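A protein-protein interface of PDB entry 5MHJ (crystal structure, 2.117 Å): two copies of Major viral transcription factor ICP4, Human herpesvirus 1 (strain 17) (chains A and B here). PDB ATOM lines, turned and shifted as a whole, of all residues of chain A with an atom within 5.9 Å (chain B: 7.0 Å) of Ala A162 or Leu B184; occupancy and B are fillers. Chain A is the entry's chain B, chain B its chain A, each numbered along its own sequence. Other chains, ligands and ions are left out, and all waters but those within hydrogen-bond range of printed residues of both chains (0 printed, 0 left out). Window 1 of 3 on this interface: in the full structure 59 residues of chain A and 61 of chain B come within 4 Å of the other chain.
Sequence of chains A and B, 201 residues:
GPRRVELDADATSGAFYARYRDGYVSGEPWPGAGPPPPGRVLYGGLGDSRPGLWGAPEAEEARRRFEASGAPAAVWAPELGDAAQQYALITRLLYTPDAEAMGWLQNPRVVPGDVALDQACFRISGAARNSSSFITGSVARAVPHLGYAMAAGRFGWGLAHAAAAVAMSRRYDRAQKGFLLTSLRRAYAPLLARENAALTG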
ATOM      1  N   GLY A 158     -11.956 -23.226   3.026  1.00  0.00           N
ATOM      2  CA  GLY A 158     -13.266 -23.849   2.979  1.00  0.00           C
ATOM      3  C   GLY A 158     -14.340 -23.103   3.744  1.00  0.00           C
ATOM      4  O   GLY A 158     -15.529 -23.302   3.471  1.00  0.00           O
ATOM      5  N   LEU A 159     -13.951 -22.248   4.696  1.00  0.00           N
ATOM      6  CA  LEU A 159     -14.945 -21.501   5.461  1.00  0.00           C
ATOM      7  C   LEU A 159     -15.801 -20.639   4.547  1.00  0.00           C
ATOM      8  O   LEU A 159     -17.025 -20.568   4.711  1.00  0.00           O
ATOM      9  CB  LEU A 159     -14.264 -20.637   6.527  1.00  0.00           C
ATOM     10  CG  LEU A 159     -15.145 -19.560   7.178  1.00  0.00           C
ATOM     11  CD1 LEU A 159     -16.314 -20.189   7.913  1.00  0.00           C
ATOM     12  CD2 LEU A 159     -14.340 -18.696   8.131  1.00  0.00           C
ATOM     13  N   ALA A 160     -15.168 -19.978   3.575  1.00  0.00           N
ATOM     14  CA  ALA A 160     -15.903 -19.146   2.631  1.00  0.00           C
ATOM     15  C   ALA A 160     -16.955 -19.953   1.884  1.00  0.00           C
ATOM     16  O   ALA A 160     -18.072 -19.474   1.661  1.00  0.00           O
ATOM     17  CB  ALA A 160     -14.928 -18.492   1.650  1.00  0.00           C
ATOM     18  N   HIS A 161     -16.617 -21.180   1.488  1.00  0.00           N
ATOM     19  CA  HIS A 161     -17.575 -22.009   0.766  1.00  0.00           C
ATOM     20  C   HIS A 161     -18.653 -22.550   1.694  1.00  0.00           C
ATOM     21  O   HIS A 161     -19.835 -22.563   1.332  1.00  0.00           O
ATOM     22  CB  HIS A 161     -16.854 -23.154   0.058  1.00  0.00           C
ATOM     23  CG  HIS A 161     -15.975 -22.703  -1.068  1.00  0.00           C
ATOM     24  ND1 HIS A 161     -16.390 -22.703  -2.383  1.00  0.00           N
ATOM     25  CD2 HIS A 161     -14.700 -22.242  -1.077  1.00  0.00           C
ATOM     26  CE1 HIS A 161     -15.411 -22.262  -3.151  1.00  0.00           C
ATOM     27  NE2 HIS A 161     -14.374 -21.976  -2.385  1.00  0.00           N
ATOM     28  N   ALA A 162     -18.270 -23.003   2.890  1.00  0.00           N
ATOM     29  CA  ALA A 162     -19.263 -23.537   3.818  1.00  0.00           C
ATOM     30  C   ALA A 162     -20.245 -22.453   4.250  1.00  0.00           C
ATOM     31  O   ALA A 162     -21.459 -22.687   4.297  1.00  0.00           O
ATOM     32  CB  ALA A 162     -18.570 -24.161   5.030  1.00  0.00           C
ATOM     33  N   ALA A 163     -19.741 -21.255   4.554  1.00  0.00           N
ATOM     34  CA  ALA A 163     -20.629 -20.152   4.904  1.00  0.00           C
ATOM     35  C   ALA A 163     -21.508 -19.754   3.724  1.00  0.00           C
ATOM     36  O   ALA A 163     -22.701 -19.480   3.896  1.00  0.00           O
ATOM     37  CB  ALA A 163     -19.816 -18.954   5.396  1.00  0.00           C
ATOM     38  N   ALA A 164     -20.938 -19.721   2.516  1.00  0.00           N
ATOM     39  CA  ALA A 164     -21.723 -19.342   1.347  1.00  0.00           C
ATOM     40  C   ALA A 164     -22.798 -20.373   1.031  1.00  0.00           C
ATOM     41  O   ALA A 164     -23.879 -20.009   0.556  1.00  0.00           O
ATOM     42  CB  ALA A 164     -20.810 -19.140   0.139  1.00  0.00           C
ATOM     43  N   ALA A 165     -22.524 -21.656   1.286  1.00  0.00           N
ATOM     44  CA  ALA A 165     -23.549 -22.677   1.101  1.00  0.00           C
ATOM     45  C   ALA A 165     -24.722 -22.449   2.045  1.00  0.00           C
ATOM     46  O   ALA A 165     -25.886 -22.557   1.641  1.00  0.00           O
ATOM     47  CB  ALA A 165     -22.953 -24.069   1.310  1.00  0.00           C
ATOM     48  N   VAL A 166     -24.431 -22.131   3.308  1.00  0.00           N
ATOM     49  CA  VAL A 166     -25.491 -21.817   4.259  1.00  0.00           C
ATOM     50  C   VAL A 166     -26.241 -20.561   3.831  1.00  0.00           C
ATOM     51  O   VAL A 166     -27.474 -20.509   3.892  1.00  0.00           O
ATOM     52  CB  VAL A 166     -24.906 -21.672   5.676  1.00  0.00           C
ATOM     53  CG1 VAL A 166     -25.950 -21.096   6.627  1.00  0.00           C
ATOM     54  CG2 VAL A 166     -24.396 -23.016   6.181  1.00  0.00           C
ATOM     55  N   ALA A 167     -25.511 -19.535   3.381  1.00  0.00           N
ATOM     56  CA  ALA A 167     -26.152 -18.281   2.997  1.00  0.00           C
ATOM     57  C   ALA A 167     -27.072 -18.457   1.797  1.00  0.00           C
ATOM     58  O   ALA A 167     -28.103 -17.782   1.703  1.00  0.00           O
ATOM     59  CB  ALA A 167     -25.095 -17.215   2.699  1.00  0.00           C
ATOM     60  N   LEU A 184     -19.541 -21.235  12.735  1.00  0.00           N
ATOM     61  CA  LEU A 184     -18.412 -21.358  11.818  1.00  0.00           C
ATOM     62  C   LEU A 184     -17.239 -20.480  12.238  1.00  0.00           C
ATOM     63  O   LEU A 184     -16.081 -20.858  12.028  1.00  0.00           O
ATOM     64  CB  LEU A 184     -18.851 -21.010  10.396  1.00  0.00           C
ATOM     65  CG  LEU A 184     -19.748 -22.051   9.726  1.00  0.00           C
ATOM     66  CD1 LEU A 184     -20.359 -21.502   8.445  1.00  0.00           C
ATOM     67  CD2 LEU A 184     -18.962 -23.327   9.455  1.00  0.00           C
ATOM     68  N   TYR A 188     -13.511 -22.241  12.886  1.00  0.00           N
ATOM     69  CA  TYR A 188     -12.415 -21.976  11.967  1.00  0.00           C
ATOM     70  C   TYR A 188     -11.363 -21.029  12.528  1.00  0.00           C
ATOM     71  O   TYR A 188     -10.268 -20.951  11.962  1.00  0.00           O
ATOM     72  CB  TYR A 188     -12.953 -21.417  10.646  1.00  0.00           C
ATOM     73  CG  TYR A 188     -13.375 -22.494   9.669  1.00  0.00           C
ATOM     74  CD1 TYR A 188     -12.472 -23.026   8.758  1.00  0.00           C
ATOM     75  CD2 TYR A 188     -14.674 -22.986   9.668  1.00  0.00           C
ATOM     76  CE1 TYR A 188     -12.853 -24.017   7.866  1.00  0.00           C
ATOM     77  CE2 TYR A 188     -15.064 -23.974   8.782  1.00  0.00           C
ATOM     78  CZ  TYR A 188     -14.149 -24.486   7.883  1.00  0.00           C
ATOM     79  OH  TYR A 188     -14.531 -25.470   7.001  1.00  0.00           O
ATOM     80  N   TYR B  95     -17.486 -38.211  11.050  1.00  0.00           N
ATOM     81  CA  TYR B  95     -16.087 -38.539  11.285  1.00  0.00           C
ATOM     82  C   TYR B  95     -15.765 -40.015  11.090  1.00  0.00           C
ATOM     83  O   TYR B  95     -14.585 -40.381  11.122  1.00  0.00           O
ATOM     84  CB  TYR B  95     -15.676 -38.119  12.704  1.00  0.00           C
ATOM     85  CG  TYR B  95     -15.512 -36.625  12.876  1.00  0.00           C
ATOM     86  CD1 TYR B  95     -16.602 -35.820  13.180  1.00  0.00           C
ATOM     87  CD2 TYR B  95     -14.269 -36.020  12.736  1.00  0.00           C
ATOM     88  CE1 TYR B  95     -16.462 -34.459  13.337  1.00  0.00           C
ATOM     89  CE2 TYR B  95     -14.118 -34.654  12.892  1.00  0.00           C
ATOM     90  CZ  TYR B  95     -15.222 -33.879  13.194  1.00  0.00           C
ATOM     91  OH  TYR B  95     -15.092 -32.521  13.353  1.00  0.00           O
ATOM     92  N   MET B 102     -21.488 -37.497   3.253  1.00  0.00           N
ATOM     93  CA  MET B 102     -21.977 -36.408   2.414  1.00  0.00           C
ATOM     94  C   MET B 102     -23.013 -36.906   1.414  1.00  0.00           C
ATOM     95  O   MET B 102     -24.003 -36.217   1.143  1.00  0.00           O
ATOM     96  CB  MET B 102     -20.812 -35.724   1.697  1.00  0.00           C
ATOM     97  CG  MET B 102     -19.841 -35.022   2.633  1.00  0.00           C
ATOM     98  SD  MET B 102     -20.563 -33.597   3.478  1.00  0.00           S
ATOM     99  CE  MET B 102     -20.482 -32.373   2.173  1.00  0.00           C
ATOM    100  N   GLY B 158     -23.665 -27.010  14.853  1.00  0.00           N
ATOM    101  CA  GLY B 158     -23.700 -26.344  13.565  1.00  0.00           C
ATOM    102  C   GLY B 158     -22.986 -27.103  12.464  1.00  0.00           C
ATOM    103  O   GLY B 158     -23.287 -26.889  11.284  1.00  0.00           O
ATOM    104  N   LEU B 159     -22.048 -27.985  12.823  1.00  0.00           N
ATOM    105  CA  LEU B 159     -21.348 -28.769  11.809  1.00  0.00           C
ATOM    106  C   LEU B 159     -22.325 -29.582  10.969  1.00  0.00           C
ATOM    107  O   LEU B 159     -22.220 -29.610   9.737  1.00  0.00           O
ATOM    108  CB  LEU B 159     -20.311 -29.688  12.465  1.00  0.00           C
ATOM    109  CG  LEU B 159     -19.740 -30.801  11.580  1.00  0.00           C
ATOM    110  CD1 LEU B 159     -18.931 -30.215  10.426  1.00  0.00           C
ATOM    111  CD2 LEU B 159     -18.889 -31.773  12.390  1.00  0.00           C
ATOM    112  N   HIS B 161     -25.392 -28.968  10.225  1.00  0.00           N
ATOM    113  CA  HIS B 161     -26.100 -28.103   9.287  1.00  0.00           C
ATOM    114  C   HIS B 161     -25.175 -27.579   8.192  1.00  0.00           C
ATOM    115  O   HIS B 161     -25.557 -27.552   7.017  1.00  0.00           O
ATOM    116  CB  HIS B 161     -26.758 -26.941  10.034  1.00  0.00           C
ATOM    117  CG  HIS B 161     -27.895 -27.361  10.916  1.00  0.00           C
ATOM    118  ND1 HIS B 161     -29.208 -27.330  10.502  1.00  0.00           N
ATOM    119  CD2 HIS B 161     -27.912 -27.825  12.189  1.00  0.00           C
ATOM    120  CE1 HIS B 161     -29.986 -27.756  11.482  1.00  0.00           C
ATOM    121  NE2 HIS B 161     -29.225 -28.060  12.518  1.00  0.00           N
ATOM    122  N   ALA B 162     -23.960 -27.156   8.557  1.00  0.00           N
ATOM    123  CA  ALA B 162     -23.020 -26.673   7.550  1.00  0.00           C
ATOM    124  C   ALA B 162     -22.631 -27.779   6.577  1.00  0.00           C
ATOM    125  O   ALA B 162     -22.553 -27.547   5.365  1.00  0.00           O
ATOM    126  CB  ALA B 162     -21.777 -26.091   8.223  1.00  0.00           C
ATOM    127  N   ALA B 163     -22.387 -28.989   7.086  1.00  0.00           N
ATOM    128  CA  ALA B 163     -22.073 -30.099   6.195  1.00  0.00           C
ATOM    129  C   ALA B 163     -23.261 -30.436   5.305  1.00  0.00           C
ATOM    130  O   ALA B 163     -23.088 -30.725   4.116  1.00  0.00           O
ATOM    131  CB  ALA B 163     -21.638 -31.319   7.004  1.00  0.00           C
ATOM    132  N   ALA B 164     -24.476 -30.393   5.858  1.00  0.00           N
ATOM    133  CA  ALA B 164     -25.655 -30.723   5.066  1.00  0.00           C
ATOM    134  C   ALA B 164     -25.931 -29.667   4.003  1.00  0.00           C
ATOM    135  O   ALA B 164     -26.403 -30.002   2.910  1.00  0.00           O
ATOM    136  CB  ALA B 164     -26.869 -30.903   5.979  1.00  0.00           C
ATOM    137  N   ALA B 165     -25.642 -28.397   4.299  1.00  0.00           N
ATOM    138  CA  ALA B 165     -25.777 -27.351   3.287  1.00  0.00           C
ATOM    139  C   ALA B 165     -24.835 -27.592   2.117  1.00  0.00           C
ATOM    140  O   ALA B 165     -25.231 -27.470   0.952  1.00  0.00           O
ATOM    141  CB  ALA B 165     -25.515 -25.978   3.906  1.00  0.00           C
ATOM    142  N   VAL B 166     -23.576 -27.925   2.406  1.00  0.00           N
ATOM    143  CA  VAL B 166     -22.641 -28.237   1.332  1.00  0.00           C
ATOM    144  C   VAL B 166     -23.102 -29.476   0.572  1.00  0.00           C
ATOM    145  O   VAL B 166     -23.109 -29.495  -0.666  1.00  0.00           O
ATOM    146  CB  VAL B 166     -21.220 -28.405   1.899  1.00  0.00           C
ATOM    147  CG1 VAL B 166     -20.283 -28.960   0.835  1.00  0.00           C
ATOM    148  CG2 VAL B 166     -20.705 -27.071   2.434  1.00  0.00           C
ATOM    149  N   TYR B 172     -21.228 -28.173  -6.242  1.00  0.00           N
ATOM    150  CA  TYR B 172     -19.970 -28.876  -6.023  1.00  0.00           C
ATOM    151  C   TYR B 172     -20.120 -30.339  -6.420  1.00  0.00           C
ATOM    152  O   TYR B 172     -21.175 -30.941  -6.198  1.00  0.00           O
ATOM    153  CB  TYR B 172     -19.530 -28.784  -4.557  1.00  0.00           C
ATOM    154  CG  TYR B 172     -19.365 -27.369  -4.052  1.00  0.00           C
ATOM    155  CD1 TYR B 172     -18.288 -26.592  -4.455  1.00  0.00           C
ATOM    156  CD2 TYR B 172     -20.283 -26.812  -3.170  1.00  0.00           C
ATOM    157  CE1 TYR B 172     -18.129 -25.303  -4.001  1.00  0.00           C
ATOM    158  CE2 TYR B 172     -20.132 -25.515  -2.709  1.00  0.00           C
ATOM    159  CZ  TYR B 172     -19.050 -24.767  -3.129  1.00  0.00           C
ATOM    160  OH  TYR B 172     -18.879 -23.477  -2.684  1.00  0.00           O
ATOM    161  N   LYS B 177     -16.880 -31.750  -2.583  1.00  0.00           N
ATOM    162  CA  LYS B 177     -17.547 -31.917  -1.296  1.00  0.00           C
ATOM    163  C   LYS B 177     -16.659 -32.646  -0.295  1.00  0.00           C
ATOM    164  O   LYS B 177     -16.683 -32.327   0.901  1.00  0.00           O
ATOM    165  CB  LYS B 177     -18.870 -32.659  -1.487  1.00  0.00           C
ATOM    166  CG  LYS B 177     -19.942 -31.819  -2.163  1.00  0.00           C
ATOM    167  CD  LYS B 177     -21.188 -32.627  -2.485  1.00  0.00           C
ATOM    168  CE  LYS B 177     -22.289 -31.722  -3.023  1.00  0.00           C
ATOM    169  NZ  LYS B 177     -23.418 -32.492  -3.611  1.00  0.00           N
ATOM    170  N   PHE B 179     -13.392 -32.473  -0.053  1.00  0.00           N
ATOM    171  CA  PHE B 179     -12.423 -31.522   0.485  1.00  0.00           C
ATOM    172  C   PHE B 179     -13.060 -30.640   1.553  1.00  0.00           C
ATOM    173  O   PHE B 179     -12.444 -30.364   2.590  1.00  0.00           O
ATOM    174  CB  PHE B 179     -11.837 -30.670  -0.642  1.00  0.00           C
ATOM    175  CG  PHE B 179     -10.972 -29.531  -0.165  1.00  0.00           C
ATOM    176  CD1 PHE B 179      -9.648 -29.745   0.191  1.00  0.00           C
ATOM    177  CD2 PHE B 179     -11.482 -28.246  -0.080  1.00  0.00           C
ATOM    178  CE1 PHE B 179      -8.851 -28.698   0.621  1.00  0.00           C
ATOM    179  CE2 PHE B 179     -10.691 -27.195   0.354  1.00  0.00           C
ATOM    180  CZ  PHE B 179      -9.375 -27.420   0.705  1.00  0.00           C
ATOM    181  N   LEU B 180     -14.299 -30.197   1.320  1.00  0.00           N
ATOM    182  CA  LEU B 180     -14.979 -29.350   2.295  1.00  0.00           C
ATOM    183  C   LEU B 180     -15.331 -30.114   3.565  1.00  0.00           C
ATOM    184  O   LEU B 180     -15.348 -29.525   4.652  1.00  0.00           O
ATOM    185  CB  LEU B 180     -16.236 -28.742   1.674  1.00  0.00           C
ATOM    186  CG  LEU B 180     -15.958 -27.650   0.642  1.00  0.00           C
ATOM    187  CD1 LEU B 180     -17.232 -27.248  -0.080  1.00  0.00           C
ATOM    188  CD2 LEU B 180     -15.309 -26.451   1.313  1.00  0.00           C
ATOM    189  N   LEU B 181     -15.623 -31.413   3.456  1.00  0.00           N
ATOM    190  CA  LEU B 181     -15.843 -32.208   4.661  1.00  0.00           C
ATOM    191  C   LEU B 181     -14.563 -32.327   5.476  1.00  0.00           C
ATOM    192  O   LEU B 181     -14.595 -32.221   6.708  1.00  0.00           O
ATOM    193  CB  LEU B 181     -16.376 -33.596   4.300  1.00  0.00           C
ATOM    194  CG  LEU B 181     -16.548 -34.576   5.465  1.00  0.00           C
ATOM    195  CD1 LEU B 181     -17.461 -34.004   6.543  1.00  0.00           C
ATOM    196  CD2 LEU B 181     -17.081 -35.913   4.969  1.00  0.00           C
ATOM    197  N   THR B 182     -13.427 -32.552   4.807  1.00  0.00           N
ATOM    198  CA  THR B 182     -12.149 -32.581   5.509  1.00  0.00           C
ATOM    199  C   THR B 182     -11.883 -31.250   6.202  1.00  0.00           C
ATOM    200  O   THR B 182     -11.447 -31.218   7.359  1.00  0.00           O
ATOM    201  CB  THR B 182     -11.018 -32.918   4.535  1.00  0.00           C
ATOM    202  OG1 THR B 182     -11.177 -34.260   4.056  1.00  0.00           O
ATOM    203  CG2 THR B 182      -9.658 -32.791   5.217  1.00  0.00           C
ATOM    204  N   SER B 183     -12.166 -30.141   5.516  1.00  0.00           N
ATOM    205  CA  SER B 183     -11.985 -28.823   6.118  1.00  0.00           C
ATOM    206  C   SER B 183     -12.898 -28.637   7.327  1.00  0.00           C
ATOM    207  O   SER B 183     -12.454 -28.190   8.392  1.00  0.00           O
ATOM    208  CB  SER B 183     -12.241 -27.734   5.074  1.00  0.00           C
ATOM    209  OG  SER B 183     -12.270 -26.448   5.670  1.00  0.00           O
ATOM    210  N   LEU B 184     -14.181 -28.983   7.183  1.00  0.00           N
ATOM    211  CA  LEU B 184     -15.114 -28.865   8.302  1.00  0.00           C
ATOM    212  C   LEU B 184     -14.710 -29.775   9.459  1.00  0.00           C
ATOM    213  O   LEU B 184     -14.791 -29.378  10.627  1.00  0.00           O
ATOM    214  CB  LEU B 184     -16.535 -29.187   7.834  1.00  0.00           C
ATOM    215  CG  LEU B 184     -17.198 -28.145   6.927  1.00  0.00           C
ATOM    216  CD1 LEU B 184     -18.353 -28.755   6.141  1.00  0.00           C
ATOM    217  CD2 LEU B 184     -17.670 -26.942   7.734  1.00  0.00           C
ATOM    218  N   ARG B 185     -14.276 -31.002   9.150  1.00  0.00           N
ATOM    219  CA  ARG B 185     -13.806 -31.920  10.185  1.00  0.00           C
ATOM    220  C   ARG B 185     -12.692 -31.295  11.019  1.00  0.00           C
ATOM    221  O   ARG B 185     -12.712 -31.365  12.253  1.00  0.00           O
ATOM    222  CB  ARG B 185     -13.315 -33.219   9.548  1.00  0.00           C
ATOM    223  CG  ARG B 185     -14.387 -34.245   9.214  1.00  0.00           C
ATOM    224  CD  ARG B 185     -13.726 -35.434   8.529  1.00  0.00           C
ATOM    225  NE  ARG B 185     -14.653 -36.488   8.126  1.00  0.00           N
ATOM    226  CZ  ARG B 185     -14.320 -37.473   7.295  1.00  0.00           C
ATOM    227  NH1 ARG B 185     -13.092 -37.522   6.791  1.00  0.00           N
ATOM    228  NH2 ARG B 185     -15.202 -38.410   6.969  1.00  0.00           N
ATOM    229  N   ARG B 186     -11.700 -30.694  10.353  1.00  0.00           N
ATOM    230  CA  ARG B 186     -10.578 -30.088  11.065  1.00  0.00           C
ATOM    231  C   ARG B 186     -11.038 -28.928  11.935  1.00  0.00           C
ATOM    232  O   ARG B 186     -10.555 -28.752  13.059  1.00  0.00           O
ATOM    233  CB  ARG B 186      -9.523 -29.599  10.070  1.00  0.00           C
ATOM    234  CG  ARG B 186      -8.636 -30.670   9.473  1.00  0.00           C
ATOM    235  CD  ARG B 186      -7.453 -30.037   8.740  1.00  0.00           C
ATOM    236  NE  ARG B 186      -6.417 -31.022   8.455  1.00  0.00           N
ATOM    237  CZ  ARG B 186      -5.147 -30.729   8.189  1.00  0.00           C
ATOM    238  NH1 ARG B 186      -4.737 -29.466   8.170  1.00  0.00           N
ATOM    239  NH2 ARG B 186      -4.285 -31.706   7.945  1.00  0.00           N
ATOM    240  N   ALA B 187     -11.956 -28.111  11.418  1.00  0.00           N
ATOM    241  CA  ALA B 187     -12.391 -26.927  12.147  1.00  0.00           C
ATOM    242  C   ALA B 187     -13.176 -27.296  13.398  1.00  0.00           C
ATOM    243  O   ALA B 187     -12.983 -26.692  14.461  1.00  0.00           O
ATOM    244  CB  ALA B 187     -13.232 -26.033  11.236  1.00  0.00           C
ATOM    245  N   TYR B 188     -14.057 -28.290  13.298  1.00  0.00           N
ATOM    246  CA  TYR B 188     -14.996 -28.567  14.376  1.00  0.00           C
ATOM    247  C   TYR B 188     -14.474 -29.559  15.405  1.00  0.00           C
ATOM    248  O   TYR B 188     -14.991 -29.580  16.527  1.00  0.00           O
ATOM    249  CB  TYR B 188     -16.323 -29.079  13.805  1.00  0.00           C
ATOM    250  CG  TYR B 188     -17.262 -27.962  13.406  1.00  0.00           C
ATOM    251  CD1 TYR B 188     -18.152 -27.412  14.323  1.00  0.00           C
ATOM    252  CD2 TYR B 188     -17.248 -27.446  12.119  1.00  0.00           C
ATOM    253  CE1 TYR B 188     -19.009 -26.381  13.962  1.00  0.00           C
ATOM    254  CE2 TYR B 188     -18.097 -26.419  11.748  1.00  0.00           C
ATOM    255  CZ  TYR B 188     -18.975 -25.889  12.671  1.00  0.00           C
ATOM    256  OH  TYR B 188     -19.817 -24.867  12.295  1.00  0.00           O
ATOM    257  N   ALA B 189     -13.469 -30.369  15.065  1.00  0.00           N
ATOM    258  CA  ALA B 189     -13.015 -31.399  15.999  1.00  0.00           C
ATOM    259  C   ALA B 189     -12.586 -30.831  17.348  1.00  0.00           C
ATOM    260  O   ALA B 189     -13.057 -31.341  18.381  1.00  0.00           O
ATOM    261  CB  ALA B 189     -11.905 -32.237  15.355  1.00  0.00           C
ATOM    262  N   PRO B 190     -11.731 -29.803  17.436  1.00  0.00           N
ATOM    263  CA  PRO B 190     -11.407 -29.271  18.770  1.00  0.00           C
ATOM    264  C   PRO B 190     -12.572 -28.543  19.418  1.00  0.00           C
ATOM    265  O   PRO B 190     -12.650 -28.501  20.651  1.00  0.00           O
ATOM    266  CB  PRO B 190     -10.224 -28.331  18.500  1.00  0.00           C
ATOM    267  CG  PRO B 190     -10.410 -27.903  17.100  1.00  0.00           C
ATOM    268  CD  PRO B 190     -10.977 -29.096  16.381  1.00  0.00           C
ATOM    269  N   LEU B 192     -15.833 -29.476  19.098  1.00  0.00           N
ATOM    270  CA  LEU B 192     -16.704 -30.523  19.619  1.00  0.00           C
ATOM    271  C   LEU B 192     -16.111 -31.161  20.870  1.00  0.00           C
ATOM    272  O   LEU B 192     -16.832 -31.443  21.833  1.00  0.00           O
ATOM    273  CB  LEU B 192     -16.954 -31.579  18.542  1.00  0.00           C
ATOM    274  CG  LEU B 192     -17.801 -31.146  17.344  1.00  0.00           C
ATOM    275  CD1 LEU B 192     -17.533 -32.055  16.154  1.00  0.00           C
ATOM    276  CD2 LEU B 192     -19.277 -31.152  17.702  1.00  0.00           C
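The side-chain hydroxyl of Tyr B172 lies within hydrogen-bond range of a ring nitrogen (ND1) of His A161. OH of Tyr A188 sits at hydrogen-bond distance from OG of Ser B183, at 2.8 Å.
Leu B180 touches Gly A158 (CD2 to CA, 3.7 Å). Gly A158 touches Ser B183. CB of His A161 touches CD2 of Leu B180, at 3.9 Å. CB of Ala A162 touches CD2 of Leu B184, 3.98 Å away. Ala A165 touches Val B166 (CB to CG2, 3.9 Å). CG2 of Val A166 touches CB of Ala B165, 3.9 Å away. Tyr B188 touches Leu A184. Leu B184 touches Tyr A188. Tyr A188 touches Ala B187.
Of the printed residues of chain B, Ala A162 touches Leu B184 (3.98 Å). Of the printed residues of chain A, Leu B184 touches Ala A162 (3.98 Å) and Tyr A188 (3.5 Å). Printed residues of chain A within 4 Å of Ala B165: Val A166. Printed residues of chain B within 4 Å of Leu A184: Tyr B188. Printed residues of chain A within 4 Å of Tyr B188: Leu A184 (3.3 Å). Of the printed residues of chain B, Val A166 touches Ala B165. Of the printed residues of chain A, Ser B183 touches Gly A158 and Tyr A188. Ala A160 touches none of the printed residues of chain B.
Of the 25 printed residues of chain B, 8 touch a printed residue of chain A. Printed residues of chain B that touch a printed residue of chain A: Ala B165, Val B166, Tyr B172, Leu B180, Ser B183, Leu B184, Ala B187 and Tyr B188. Among the printed residues, 11 pairs touch across the chains. Among the printed residues, no Asp or Glu carboxylate lies within 4 Å of a Lys or Arg side-chain nitrogen of the other chain.
Ala A162 touches Leu B184, but with the chains exchanged Leu A184 does not touch Ala B162 (4.1 Å). Ala A165 touches Val B166, and with the chains exchanged Val A166 touches Ala B165. Leu A184 touches Tyr B188, and with the chains exchanged Tyr A188 touches Leu B184. Of the 11 pairs that touch across the chains among the printed residues, 4 have their exchanged pair printed and touching as well.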
